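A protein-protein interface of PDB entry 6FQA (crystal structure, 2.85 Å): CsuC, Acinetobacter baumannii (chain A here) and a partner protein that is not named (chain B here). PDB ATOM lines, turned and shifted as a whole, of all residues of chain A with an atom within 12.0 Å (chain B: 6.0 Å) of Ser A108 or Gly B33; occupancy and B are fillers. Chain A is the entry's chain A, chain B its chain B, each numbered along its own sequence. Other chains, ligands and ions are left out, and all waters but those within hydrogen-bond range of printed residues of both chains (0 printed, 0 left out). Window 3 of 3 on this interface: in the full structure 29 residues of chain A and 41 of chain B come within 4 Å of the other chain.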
ATOM      1  N   SER A 108      22.230   9.114 -22.538  1.00  0.00           N
ATOM      2  CA  SER A 108      21.266   8.701 -21.517  1.00  0.00           C
ATOM      3  C   SER A 108      20.709   7.267 -21.733  1.00  0.00           C
ATOM      4  O   SER A 108      19.869   7.042 -22.611  1.00  0.00           O
ATOM      5  CB  SER A 108      20.121   9.713 -21.465  1.00  0.00           C
ATOM      6  OG  SER A 108      19.175   9.379 -20.466  1.00  0.00           O
ATOM      7  N   LYS A 109      21.166   6.312 -20.911  1.00  0.00           N
ATOM      8  CA  LYS A 109      20.912   4.883 -21.094  1.00  0.00           C
ATOM      9  C   LYS A 109      20.105   4.299 -19.936  1.00  0.00           C
ATOM     10  O   LYS A 109      20.032   4.873 -18.846  1.00  0.00           O
ATOM     11  CB  LYS A 109      22.225   4.078 -21.196  1.00  0.00           C
ATOM     12  CG  LYS A 109      23.253   4.576 -22.197  1.00  0.00           C
ATOM     13  CD  LYS A 109      24.653   4.670 -21.563  1.00  0.00           C
ATOM     14  CE  LYS A 109      25.017   3.427 -20.752  1.00  0.00           C
ATOM     15  NZ  LYS A 109      26.361   3.535 -20.126  1.00  0.00           N
ATOM     16  N   VAL A 110      19.519   3.125 -20.184  1.00  0.00           N
ATOM     17  CA  VAL A 110      18.921   2.292 -19.139  1.00  0.00           C
ATOM     18  C   VAL A 110      19.180   0.823 -19.482  1.00  0.00           C
ATOM     19  O   VAL A 110      18.939   0.382 -20.611  1.00  0.00           O
ATOM     20  CB  VAL A 110      17.415   2.578 -18.952  1.00  0.00           C
ATOM     21  CG1 VAL A 110      16.659   2.427 -20.253  1.00  0.00           C
ATOM     22  CG2 VAL A 110      16.825   1.688 -17.877  1.00  0.00           C
ATOM     23  N   SER A 111      19.679   0.071 -18.506  1.00  0.00           N
ATOM     24  CA  SER A 111      20.309  -1.223 -18.729  1.00  0.00           C
ATOM     25  C   SER A 111      19.619  -2.323 -17.925  1.00  0.00           C
ATOM     26  O   SER A 111      18.854  -2.062 -16.993  1.00  0.00           O
ATOM     27  CB  SER A 111      21.790  -1.142 -18.363  1.00  0.00           C
ATOM     28  OG  SER A 111      21.955  -0.349 -17.192  1.00  0.00           O
ATOM     29  N   PHE A 112      19.913  -3.572 -18.273  1.00  0.00           N
ATOM     30  CA  PHE A 112      19.151  -4.700 -17.752  1.00  0.00           C
ATOM     31  C   PHE A 112      20.018  -5.626 -16.917  1.00  0.00           C
ATOM     32  O   PHE A 112      21.093  -6.043 -17.355  1.00  0.00           O
ATOM     33  CB  PHE A 112      18.505  -5.495 -18.885  1.00  0.00           C
ATOM     34  CG  PHE A 112      17.484  -4.725 -19.644  1.00  0.00           C
ATOM     35  CD1 PHE A 112      16.331  -4.302 -19.026  1.00  0.00           C
ATOM     36  CD2 PHE A 112      17.684  -4.413 -20.976  1.00  0.00           C
ATOM     37  CE1 PHE A 112      15.393  -3.588 -19.727  1.00  0.00           C
ATOM     38  CE2 PHE A 112      16.756  -3.700 -21.685  1.00  0.00           C
ATOM     39  CZ  PHE A 112      15.605  -3.290 -21.066  1.00  0.00           C
ATOM     40  N   LEU B  30      18.871  -0.272 -23.495  1.00  0.00           N
ATOM     41  CA  LEU B  30      17.953   0.699 -24.091  1.00  0.00           C
ATOM     42  C   LEU B  30      18.618   2.063 -24.143  1.00  0.00           C
ATOM     43  O   LEU B  30      18.647   2.790 -23.147  1.00  0.00           O
ATOM     44  CB  LEU B  30      16.668   0.783 -23.285  1.00  0.00           C
ATOM     45  CG  LEU B  30      15.575  -0.222 -23.580  1.00  0.00           C
ATOM     46  CD1 LEU B  30      14.339   0.137 -22.783  1.00  0.00           C
ATOM     47  CD2 LEU B  30      15.291  -0.214 -25.069  1.00  0.00           C
ATOM     48  N   ASN B  31      19.126   2.429 -25.314  1.00  0.00           N
ATOM     49  CA  ASN B  31      19.762   3.722 -25.510  1.00  0.00           C
ATOM     50  C   ASN B  31      18.734   4.668 -26.125  1.00  0.00           C
ATOM     51  O   ASN B  31      18.373   4.529 -27.300  1.00  0.00           O
ATOM     52  CB  ASN B  31      21.004   3.587 -26.388  1.00  0.00           C
ATOM     53  CG  ASN B  31      21.919   4.785 -26.271  1.00  0.00           C
ATOM     54  OD1 ASN B  31      21.714   5.645 -25.414  1.00  0.00           O
ATOM     55  ND2 ASN B  31      22.943   4.843 -27.115  1.00  0.00           N
ATOM     56  N   PHE B  32      18.263   5.629 -25.324  1.00  0.00           N
ATOM     57  CA  PHE B  32      17.272   6.582 -25.805  1.00  0.00           C
ATOM     58  C   PHE B  32      17.899   7.718 -26.601  1.00  0.00           C
ATOM     59  O   PHE B  32      17.255   8.261 -27.507  1.00  0.00           O
ATOM     60  CB  PHE B  32      16.471   7.151 -24.631  1.00  0.00           C
ATOM     61  CG  PHE B  32      15.314   6.286 -24.197  1.00  0.00           C
ATOM     62  CD1 PHE B  32      14.205   6.125 -25.018  1.00  0.00           C
ATOM     63  CD2 PHE B  32      15.332   5.640 -22.971  1.00  0.00           C
ATOM     64  CE1 PHE B  32      13.143   5.336 -24.631  1.00  0.00           C
ATOM     65  CE2 PHE B  32      14.270   4.848 -22.574  1.00  0.00           C
ATOM     66  CZ  PHE B  32      13.172   4.699 -23.406  1.00  0.00           C
ATOM     67  N   GLY B  33      19.136   8.086 -26.288  1.00  0.00           N
ATOM     68  CA  GLY B  33      19.746   9.248 -26.896  1.00  0.00           C
ATOM     69  C   GLY B  33      20.040  10.341 -25.894  1.00  0.00           C
ATOM     70  O   GLY B  33      20.957  10.212 -25.073  1.00  0.00           O
ATOM     71  N   LYS B  34      19.262  11.422 -25.948  1.00  0.00           N
ATOM     72  CA  LYS B  34      19.484  12.578 -25.094  1.00  0.00           C
ATOM     73  C   LYS B  34      18.170  13.034 -24.486  1.00  0.00           C
ATOM     74  O   LYS B  34      17.149  13.111 -25.175  1.00  0.00           O
ATOM     75  CB  LYS B  34      20.137  13.725 -25.869  1.00  0.00           C
ATOM     76  CG  LYS B  34      19.312  14.277 -27.012  1.00  0.00           C
ATOM     77  CD  LYS B  34      19.831  15.647 -27.403  1.00  0.00           C
ATOM     78  CE  LYS B  34      19.771  16.599 -26.221  1.00  0.00           C
ATOM     79  NZ  LYS B  34      20.768  17.696 -26.331  1.00  0.00           N
ATOM     80  N   THR B  35      18.205  13.321 -23.192  1.00  0.00           N
ATOM     81  CA  THR B  35      17.060  13.827 -22.451  1.00  0.00           C
ATOM     82  C   THR B  35      17.422  15.125 -21.736  1.00  0.00           C
ATOM     83  O   THR B  35      16.935  15.406 -20.637  1.00  0.00           O
ATOM     84  CB  THR B  35      16.553  12.774 -21.467  1.00  0.00           C
ATOM     85  OG1 THR B  35      15.647  13.369 -20.531  1.00  0.00           O
ATOM     86  CG2 THR B  35      17.708  12.166 -20.721  1.00  0.00           C
ATOM     87  N   LEU B  43      10.168   9.728 -26.747  1.00  0.00           N
ATOM     88  CA  LEU B  43      11.432   9.174 -27.214  1.00  0.00           C
ATOM     89  C   LEU B  43      11.369   7.654 -27.313  1.00  0.00           C
ATOM     90  O   LEU B  43      10.836   6.985 -26.426  1.00  0.00           O
ATOM     91  CB  LEU B  43      12.578   9.569 -26.281  1.00  0.00           C
ATOM     92  CG  LEU B  43      13.125  11.001 -26.242  1.00  0.00           C
ATOM     93  CD1 LEU B  43      12.084  12.035 -25.810  1.00  0.00           C
ATOM     94  CD2 LEU B  43      14.376  11.074 -25.359  1.00  0.00           C
ATOM     95  N   LEU B  82      15.074   7.823 -14.615  1.00  0.00           N
ATOM     96  CA  LEU B  82      16.513   8.011 -14.767  1.00  0.00           C
ATOM     97  C   LEU B  82      17.044   9.054 -13.772  1.00  0.00           C
ATOM     98  O   LEU B  82      16.295   9.689 -13.026  1.00  0.00           O
ATOM     99  CB  LEU B  82      16.864   8.410 -16.201  1.00  0.00           C
ATOM    100  CG  LEU B  82      16.537   7.404 -17.307  1.00  0.00           C
ATOM    101  CD1 LEU B  82      15.216   7.703 -17.955  1.00  0.00           C
ATOM    102  CD2 LEU B  82      17.648   7.378 -18.356  1.00  0.00           C
ATOM    103  N   VAL B  91      14.179  11.936 -14.906  1.00  0.00           N
ATOM    104  CA  VAL B  91      13.174  11.883 -15.965  1.00  0.00           C
ATOM    105  C   VAL B  91      12.575  10.475 -16.009  1.00  0.00           C
ATOM    106  O   VAL B  91      13.308   9.479 -15.983  1.00  0.00           O
ATOM    107  CB  VAL B  91      13.763  12.302 -17.330  1.00  0.00           C
ATOM    108  CG1 VAL B  91      15.287  12.194 -17.316  1.00  0.00           C
ATOM    109  CG2 VAL B  91      13.145  11.500 -18.482  1.00  0.00           C
ATOM    110  N   GLY B 140      23.525  16.050 -18.935  1.00  0.00           N
ATOM    111  CA  GLY B 140      24.138  15.476 -20.122  1.00  0.00           C
ATOM    112  C   GLY B 140      23.857  14.001 -20.407  1.00  0.00           C
ATOM    113  O   GLY B 140      23.542  13.653 -21.546  1.00  0.00           O
ATOM    114  N   ASP B 141      23.970  13.150 -19.379  1.00  0.00           N
ATOM    115  CA  ASP B 141      23.847  11.691 -19.490  1.00  0.00           C
ATOM    116  C   ASP B 141      23.108  11.152 -18.268  1.00  0.00           C
ATOM    117  O   ASP B 141      23.603  11.278 -17.145  1.00  0.00           O
ATOM    118  CB  ASP B 141      25.216  11.000 -19.619  1.00  0.00           C
ATOM    119  CG  ASP B 141      25.901  11.246 -20.964  1.00  0.00           C
ATOM    120  OD1 ASP B 141      25.241  11.687 -21.929  1.00  0.00           O
ATOM    121  OD2 ASP B 141      27.117  10.974 -21.059  1.00  0.00           O
ATOM    122  N   TYR B 142      21.936  10.550 -18.483  1.00  0.00           N
ATOM    123  CA  TYR B 142      21.090   9.998 -17.426  1.00  0.00           C
ATOM    124  C   TYR B 142      21.121   8.470 -17.445  1.00  0.00           C
ATOM    125  O   TYR B 142      21.443   7.861 -18.465  1.00  0.00           O
ATOM    126  CB  TYR B 142      19.641  10.472 -17.583  1.00  0.00           C
ATOM    127  CG  TYR B 142      19.422  11.955 -17.388  1.00  0.00           C
ATOM    128  CD1 TYR B 142      19.897  12.880 -18.316  1.00  0.00           C
ATOM    129  CD2 TYR B 142      18.723  12.431 -16.288  1.00  0.00           C
ATOM    130  CE1 TYR B 142      19.687  14.231 -18.146  1.00  0.00           C
ATOM    131  CE2 TYR B 142      18.511  13.784 -16.108  1.00  0.00           C
ATOM    132  CZ  TYR B 142      18.995  14.678 -17.038  1.00  0.00           C
ATOM    133  OH  TYR B 142      18.787  16.027 -16.858  1.00  0.00           O
ATOM    134  N   LYS B 143      20.797   7.841 -16.304  1.00  0.00           N
ATOM    135  CA  LYS B 143      20.896   6.382 -16.205  1.00  0.00           C
ATOM    136  C   LYS B 143      19.817   5.763 -15.316  1.00  0.00           C
ATOM    137  O   LYS B 143      19.273   6.399 -14.414  1.00  0.00           O
ATOM    138  CB  LYS B 143      22.270   5.947 -15.663  1.00  0.00           C
ATOM    139  CG  LYS B 143      23.455   6.322 -16.540  1.00  0.00           C
ATOM    140  CD  LYS B 143      24.512   5.238 -16.537  1.00  0.00           C
ATOM    141  CE  LYS B 143      25.822   5.752 -17.097  1.00  0.00           C
ATOM    142  NZ  LYS B 143      26.546   6.569 -16.078  1.00  0.00           N
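Among the printed residues, merely in contact across the chains: Ser A108 with Asn B31, Ser A108 with Thr B35, Ser A108 with Leu B82, Lys A109 with Leu B30, Lys A109 with Asn B31, Lys A109 with Leu B82, Lys A109 with Lys B143 and Phe A112 with Leu B30.
Of the 5 printed residues of chain A, 4 touch a printed residue of chain B.
Among the printed residues, 13 pairs touch across the chains.
Among the printed residues, no Asp or Glu carboxylate lies within 4 Å of a Lys or Arg side-chain nitrogen of the other chain.
N of Leu B82 sits at hydrogen-bond distance from O of Val B91 (2.8 Å).
Of the printed residues of chain B, Ser A108 touches Asn B31, Phe B32, Gly B33, Thr B35, Leu B82 and Tyr B142.
Of the printed residues of chain B, Lys A109 touches Leu B30 (3.7 Å), Asn B31 (3.7 Å), Leu B82 (3.5 Å), Tyr B142 (2.9 Å) and Lys B143 (3.2 Å).
Of the printed residues of chain B, Phe A112 touches Leu B30.
Of chain A, only Ser A108 comes within 4 Å of Phe B32.
Gly B33 touches just one residue of chain A: Ser A108.
No residue of chain A comes within 4 Å of Lys B34.
Val B91 touches none of the printed residues of chain A.
No residue of chain A comes within 4 Å of Gly B140.
Asp B141 touches none of the printed residues of chain A.
Of chain A, only Ser A108 and Lys A109 come within 4 Å of Tyr B142.
Of chain A, only Lys A109 (3.2 Å) comes within 4 Å of Lys B143.
The nearest residue of chain A that does not touch Gly B33 is Lys A109 (5.7 Å).
The nearest printed residue of chain B that does not touch Val A110 is Phe B32 (4.1 Å).
The backbone carbonyl oxygen (O) of Ser A108 lies within hydrogen-bond range of the backbone NH (N) of Phe B32 (3.5 Å).
The backbone NH (N) of Ser A108 lies within hydrogen-bond range of the backbone carbonyl oxygen (O) of Gly B33, at 3.0 Å.
O of Tyr B142 sits close to OG of Ser A108.
N of Lys A109 is in hydrogen-bond range of O of Tyr B142, at 2.9 Å.
O of Val A110 is in hydrogen-bond range of N of Leu B30 (3.0 Å).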
